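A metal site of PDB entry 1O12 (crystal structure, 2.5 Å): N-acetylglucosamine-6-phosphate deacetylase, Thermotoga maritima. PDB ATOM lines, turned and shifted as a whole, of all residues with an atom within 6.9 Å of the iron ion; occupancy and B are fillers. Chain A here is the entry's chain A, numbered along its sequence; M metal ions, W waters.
NE2 of His 139 lies close to OE2 of Glu 127 (2.5 Å). OE1 of Glu 127 sits at hydrogen-bond distance from NE2 of His 61, at 2.7 Å. A ring nitrogen (NE2) of His 63 sits close to the side-chain carboxylate (OE1) of Glu 127, at 3.5 Å. A ring nitrogen (ND1) of His 188 is in hydrogen-bond range of the backbone carbonyl oxygen (O) of Lys 135 (2.9 Å). ND1 of His 209 lies within hydrogen-bond range of O of Asn 212.
Residues that only touch the iron ion: His 139. Of the 15 residues printed, 4 come within 4 Å of the iron ion.
OE2 of Glu 127 is bound to the iron ion, at 2.2 Å. NE2 of His 188 binds the iron ion (2.2 Å). The iron ion is bound by a ring nitrogen (NE2) of His 209, at 2.3 Å. Slightly farther from the iron ion lies water W2 (2.8 Å). Slightly farther from the iron ion lies water W1 (2.8 Å).
Water W2 lies within hydrogen-bond range of the side-chain carboxylate of Asp 267 (3.1 Å), the side-chain carboxylate of Glu 127 (3.2 Å) and a ring nitrogen (NE2) of His 63 (3.3 Å).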
ATOM      1  N   HIS A  61     -39.296  -5.823  25.531  1.00  0.00           N
ATOM      2  CA  HIS A  61     -38.126  -5.109  25.998  1.00  0.00           C
ATOM      3  C   HIS A  61     -38.202  -3.617  25.750  1.00  0.00           C
ATOM      4  O   HIS A  61     -37.777  -3.140  24.702  1.00  0.00           O
ATOM      5  CB  HIS A  61     -36.872  -5.677  25.302  1.00  0.00           C
ATOM      6  CG  HIS A  61     -35.598  -5.301  25.971  1.00  0.00           C
ATOM      7  ND1 HIS A  61     -34.411  -5.939  25.702  1.00  0.00           N
ATOM      8  CD2 HIS A  61     -35.310  -4.358  26.904  1.00  0.00           C
ATOM      9  CE1 HIS A  61     -33.439  -5.406  26.439  1.00  0.00           C
ATOM     10  NE2 HIS A  61     -33.967  -4.448  27.175  1.00  0.00           N
ATOM     11  N   HIS A  63     -37.881   0.117  28.259  1.00  0.00           N
ATOM     12  CA  HIS A  63     -37.665   0.754  29.564  1.00  0.00           C
ATOM     13  C   HIS A  63     -38.648   1.887  29.869  1.00  0.00           C
ATOM     14  O   HIS A  63     -39.187   1.987  30.967  1.00  0.00           O
ATOM     15  CB  HIS A  63     -36.233   1.324  29.617  1.00  0.00           C
ATOM     16  CG  HIS A  63     -35.188   0.295  29.306  1.00  0.00           C
ATOM     17  ND1 HIS A  63     -34.751  -0.616  30.233  1.00  0.00           N
ATOM     18  CD2 HIS A  63     -34.578  -0.026  28.137  1.00  0.00           C
ATOM     19  CE1 HIS A  63     -33.926  -1.475  29.650  1.00  0.00           C
ATOM     20  NE2 HIS A  63     -33.810  -1.138  28.377  1.00  0.00           N
ATOM     21  N   GLU A 127     -33.973  -6.920  33.400  1.00  0.00           N
ATOM     22  CA  GLU A 127     -32.718  -6.900  32.658  1.00  0.00           C
ATOM     23  C   GLU A 127     -31.657  -6.542  33.682  1.00  0.00           C
ATOM     24  O   GLU A 127     -31.543  -5.392  34.082  1.00  0.00           O
ATOM     25  CB  GLU A 127     -32.741  -5.842  31.556  1.00  0.00           C
ATOM     26  CG  GLU A 127     -31.711  -6.095  30.448  1.00  0.00           C
ATOM     27  CD  GLU A 127     -31.334  -4.860  29.683  1.00  0.00           C
ATOM     28  OE1 GLU A 127     -32.217  -4.142  29.154  1.00  0.00           O
ATOM     29  OE2 GLU A 127     -30.141  -4.585  29.593  1.00  0.00           O
ATOM     30  N   ILE A 131     -25.707  -9.849  35.544  1.00  0.00           N
ATOM     31  CA  ILE A 131     -25.001  -9.846  34.299  1.00  0.00           C
ATOM     32  C   ILE A 131     -23.516  -9.706  34.489  1.00  0.00           C
ATOM     33  O   ILE A 131     -23.019  -9.628  35.604  1.00  0.00           O
ATOM     34  CB  ILE A 131     -25.556  -8.732  33.367  1.00  0.00           C
ATOM     35  CG1 ILE A 131     -25.485  -7.363  34.051  1.00  0.00           C
ATOM     36  CG2 ILE A 131     -26.982  -9.080  32.973  1.00  0.00           C
ATOM     37  CD1 ILE A 131     -26.066  -6.208  33.204  1.00  0.00           C
ATOM     38  N   LYS A 135     -19.539  -6.670  30.109  1.00  0.00           N
ATOM     39  CA  LYS A 135     -20.449  -6.373  29.028  1.00  0.00           C
ATOM     40  C   LYS A 135     -21.656  -5.689  29.656  1.00  0.00           C
ATOM     41  O   LYS A 135     -22.795  -5.909  29.270  1.00  0.00           O
ATOM     42  CB  LYS A 135     -20.866  -7.664  28.304  1.00  0.00           C
ATOM     43  CG  LYS A 135     -19.811  -8.206  27.345  1.00  0.00           C
ATOM     44  CD  LYS A 135     -19.575  -7.207  26.232  1.00  0.00           C
ATOM     45  CE  LYS A 135     -18.506  -7.656  25.282  1.00  0.00           C
ATOM     46  NZ  LYS A 135     -18.265  -6.636  24.218  1.00  0.00           N
ATOM     47  N   LYS A 136     -21.385  -4.857  30.653  1.00  0.00           N
ATOM     48  CA  LYS A 136     -22.418  -4.142  31.378  1.00  0.00           C
ATOM     49  C   LYS A 136     -23.146  -3.101  30.553  1.00  0.00           C
ATOM     50  O   LYS A 136     -24.340  -2.887  30.741  1.00  0.00           O
ATOM     51  CB  LYS A 136     -21.801  -3.454  32.599  1.00  0.00           C
ATOM     52  CG  LYS A 136     -20.855  -2.301  32.262  1.00  0.00           C
ATOM     53  CD  LYS A 136     -20.162  -1.779  33.516  1.00  0.00           C
ATOM     54  CE  LYS A 136     -19.229  -0.591  33.181  1.00  0.00           C
ATOM     55  NZ  LYS A 136     -19.981   0.675  32.851  1.00  0.00           N
ATOM     56  N   GLY A 137     -22.401  -2.437  29.670  1.00  0.00           N
ATOM     57  CA  GLY A 137     -22.951  -1.399  28.817  1.00  0.00           C
ATOM     58  C   GLY A 137     -24.206  -0.676  29.276  1.00  0.00           C
ATOM     59  O   GLY A 137     -25.328  -1.184  29.138  1.00  0.00           O
ATOM     60  N   ALA A 138     -24.053   0.519  29.815  1.00  0.00           N
ATOM     61  CA  ALA A 138     -25.217   1.292  30.249  1.00  0.00           C
ATOM     62  C   ALA A 138     -25.837   0.813  31.561  1.00  0.00           C
ATOM     63  O   ALA A 138     -26.738   1.459  32.084  1.00  0.00           O
ATOM     64  CB  ALA A 138     -26.271   1.310  29.153  1.00  0.00           C
ATOM     65  N   HIS A 139     -25.381  -0.314  32.098  1.00  0.00           N
ATOM     66  CA  HIS A 139     -25.922  -0.761  33.377  1.00  0.00           C
ATOM     67  C   HIS A 139     -24.997  -0.223  34.465  1.00  0.00           C
ATOM     68  O   HIS A 139     -23.778  -0.136  34.279  1.00  0.00           O
ATOM     69  CB  HIS A 139     -25.991  -2.302  33.447  1.00  0.00           C
ATOM     70  CG  HIS A 139     -27.235  -2.882  32.835  1.00  0.00           C
ATOM     71  ND1 HIS A 139     -28.414  -3.021  33.528  1.00  0.00           N
ATOM     72  CD2 HIS A 139     -27.486  -3.358  31.584  1.00  0.00           C
ATOM     73  CE1 HIS A 139     -29.337  -3.552  32.741  1.00  0.00           C
ATOM     74  NE2 HIS A 139     -28.796  -3.763  31.558  1.00  0.00           N
ATOM     75  N   THR A 163     -33.127 -11.243  32.016  1.00  0.00           N
ATOM     76  CA  THR A 163     -31.896 -11.361  31.224  1.00  0.00           C
ATOM     77  C   THR A 163     -30.651 -11.540  32.119  1.00  0.00           C
ATOM     78  O   THR A 163     -30.337 -10.681  32.948  1.00  0.00           O
ATOM     79  CB  THR A 163     -31.665 -10.124  30.335  1.00  0.00           C
ATOM     80  OG1 THR A 163     -32.691 -10.051  29.346  1.00  0.00           O
ATOM     81  CG2 THR A 163     -30.306 -10.230  29.619  1.00  0.00           C
ATOM     82  N   HIS A 188     -25.625  -9.621  27.925  1.00  0.00           N
ATOM     83  CA  HIS A 188     -24.617  -8.926  28.741  1.00  0.00           C
ATOM     84  C   HIS A 188     -23.680  -9.951  29.339  1.00  0.00           C
ATOM     85  O   HIS A 188     -23.465  -9.982  30.540  1.00  0.00           O
ATOM     86  CB  HIS A 188     -25.311  -8.131  29.830  1.00  0.00           C
ATOM     87  CG  HIS A 188     -26.153  -7.019  29.298  1.00  0.00           C
ATOM     88  ND1 HIS A 188     -25.601  -5.878  28.740  1.00  0.00           N
ATOM     89  CD2 HIS A 188     -27.498  -6.881  29.194  1.00  0.00           C
ATOM     90  CE1 HIS A 188     -26.574  -5.075  28.327  1.00  0.00           C
ATOM     91  NE2 HIS A 188     -27.731  -5.665  28.599  1.00  0.00           N
ATOM     92  N   THR A 208     -30.815 -11.788  24.492  1.00  0.00           N
ATOM     93  CA  THR A 208     -31.225 -10.377  24.664  1.00  0.00           C
ATOM     94  C   THR A 208     -30.427  -9.432  23.760  1.00  0.00           C
ATOM     95  O   THR A 208     -29.191  -9.490  23.711  1.00  0.00           O
ATOM     96  CB  THR A 208     -31.148  -9.970  26.203  1.00  0.00           C
ATOM     97  OG1 THR A 208     -32.050 -10.795  26.944  1.00  0.00           O
ATOM     98  CG2 THR A 208     -31.521  -8.502  26.449  1.00  0.00           C
ATOM     99  N   HIS A 209     -31.164  -8.553  23.083  1.00  0.00           N
ATOM    100  CA  HIS A 209     -30.656  -7.634  22.056  1.00  0.00           C
ATOM    101  C   HIS A 209     -29.320  -8.063  21.427  1.00  0.00           C
ATOM    102  O   HIS A 209     -28.251  -7.524  21.741  1.00  0.00           O
ATOM    103  CB  HIS A 209     -30.638  -6.151  22.492  1.00  0.00           C
ATOM    104  CG  HIS A 209     -29.932  -5.898  23.784  1.00  0.00           C
ATOM    105  ND1 HIS A 209     -28.769  -6.538  24.129  1.00  0.00           N
ATOM    106  CD2 HIS A 209     -30.214  -5.051  24.799  1.00  0.00           C
ATOM    107  CE1 HIS A 209     -28.376  -6.107  25.321  1.00  0.00           C
ATOM    108  NE2 HIS A 209     -29.238  -5.209  25.743  1.00  0.00           N
ATOM    109  N   ASN A 212     -25.564  -7.025  20.585  1.00  0.00           N
ATOM    110  CA  ASN A 212     -24.976  -6.049  21.506  1.00  0.00           C
ATOM    111  C   ASN A 212     -24.772  -6.674  22.889  1.00  0.00           C
ATOM    112  O   ASN A 212     -25.641  -7.402  23.391  1.00  0.00           O
ATOM    113  CB  ASN A 212     -25.855  -4.803  21.639  1.00  0.00           C
ATOM    114  CG  ASN A 212     -26.433  -4.324  20.301  1.00  0.00           C
ATOM    115  OD1 ASN A 212     -27.628  -4.543  20.006  1.00  0.00           O
ATOM    116  ND2 ASN A 212     -25.604  -3.662  19.482  1.00  0.00           N
ATOM    117  N   ASP A 267     -36.328  -1.532  23.123  1.00  0.00           N
ATOM    118  CA  ASP A 267     -35.241  -1.154  24.034  1.00  0.00           C
ATOM    119  C   ASP A 267     -35.276   0.358  24.173  1.00  0.00           C
ATOM    120  O   ASP A 267     -34.271   1.029  24.408  1.00  0.00           O
ATOM    121  CB  ASP A 267     -33.871  -1.618  23.479  1.00  0.00           C
ATOM    122  CG  ASP A 267     -32.709  -1.485  24.508  1.00  0.00           C
ATOM    123  OD1 ASP A 267     -32.845  -1.875  25.710  1.00  0.00           O
ATOM    124  OD2 ASP A 267     -31.620  -1.015  24.105  1.00  0.00           O
HETATM  125 FE    FE M   1     -29.045  -4.068  27.758  1.00  0.00          FE
HETATM  126  O   HOH W   1     -27.746  -1.552  27.812  1.00  0.00           O
HETATM  127  O   HOH W   2     -30.624  -1.755  27.829  1.00  0.00           O
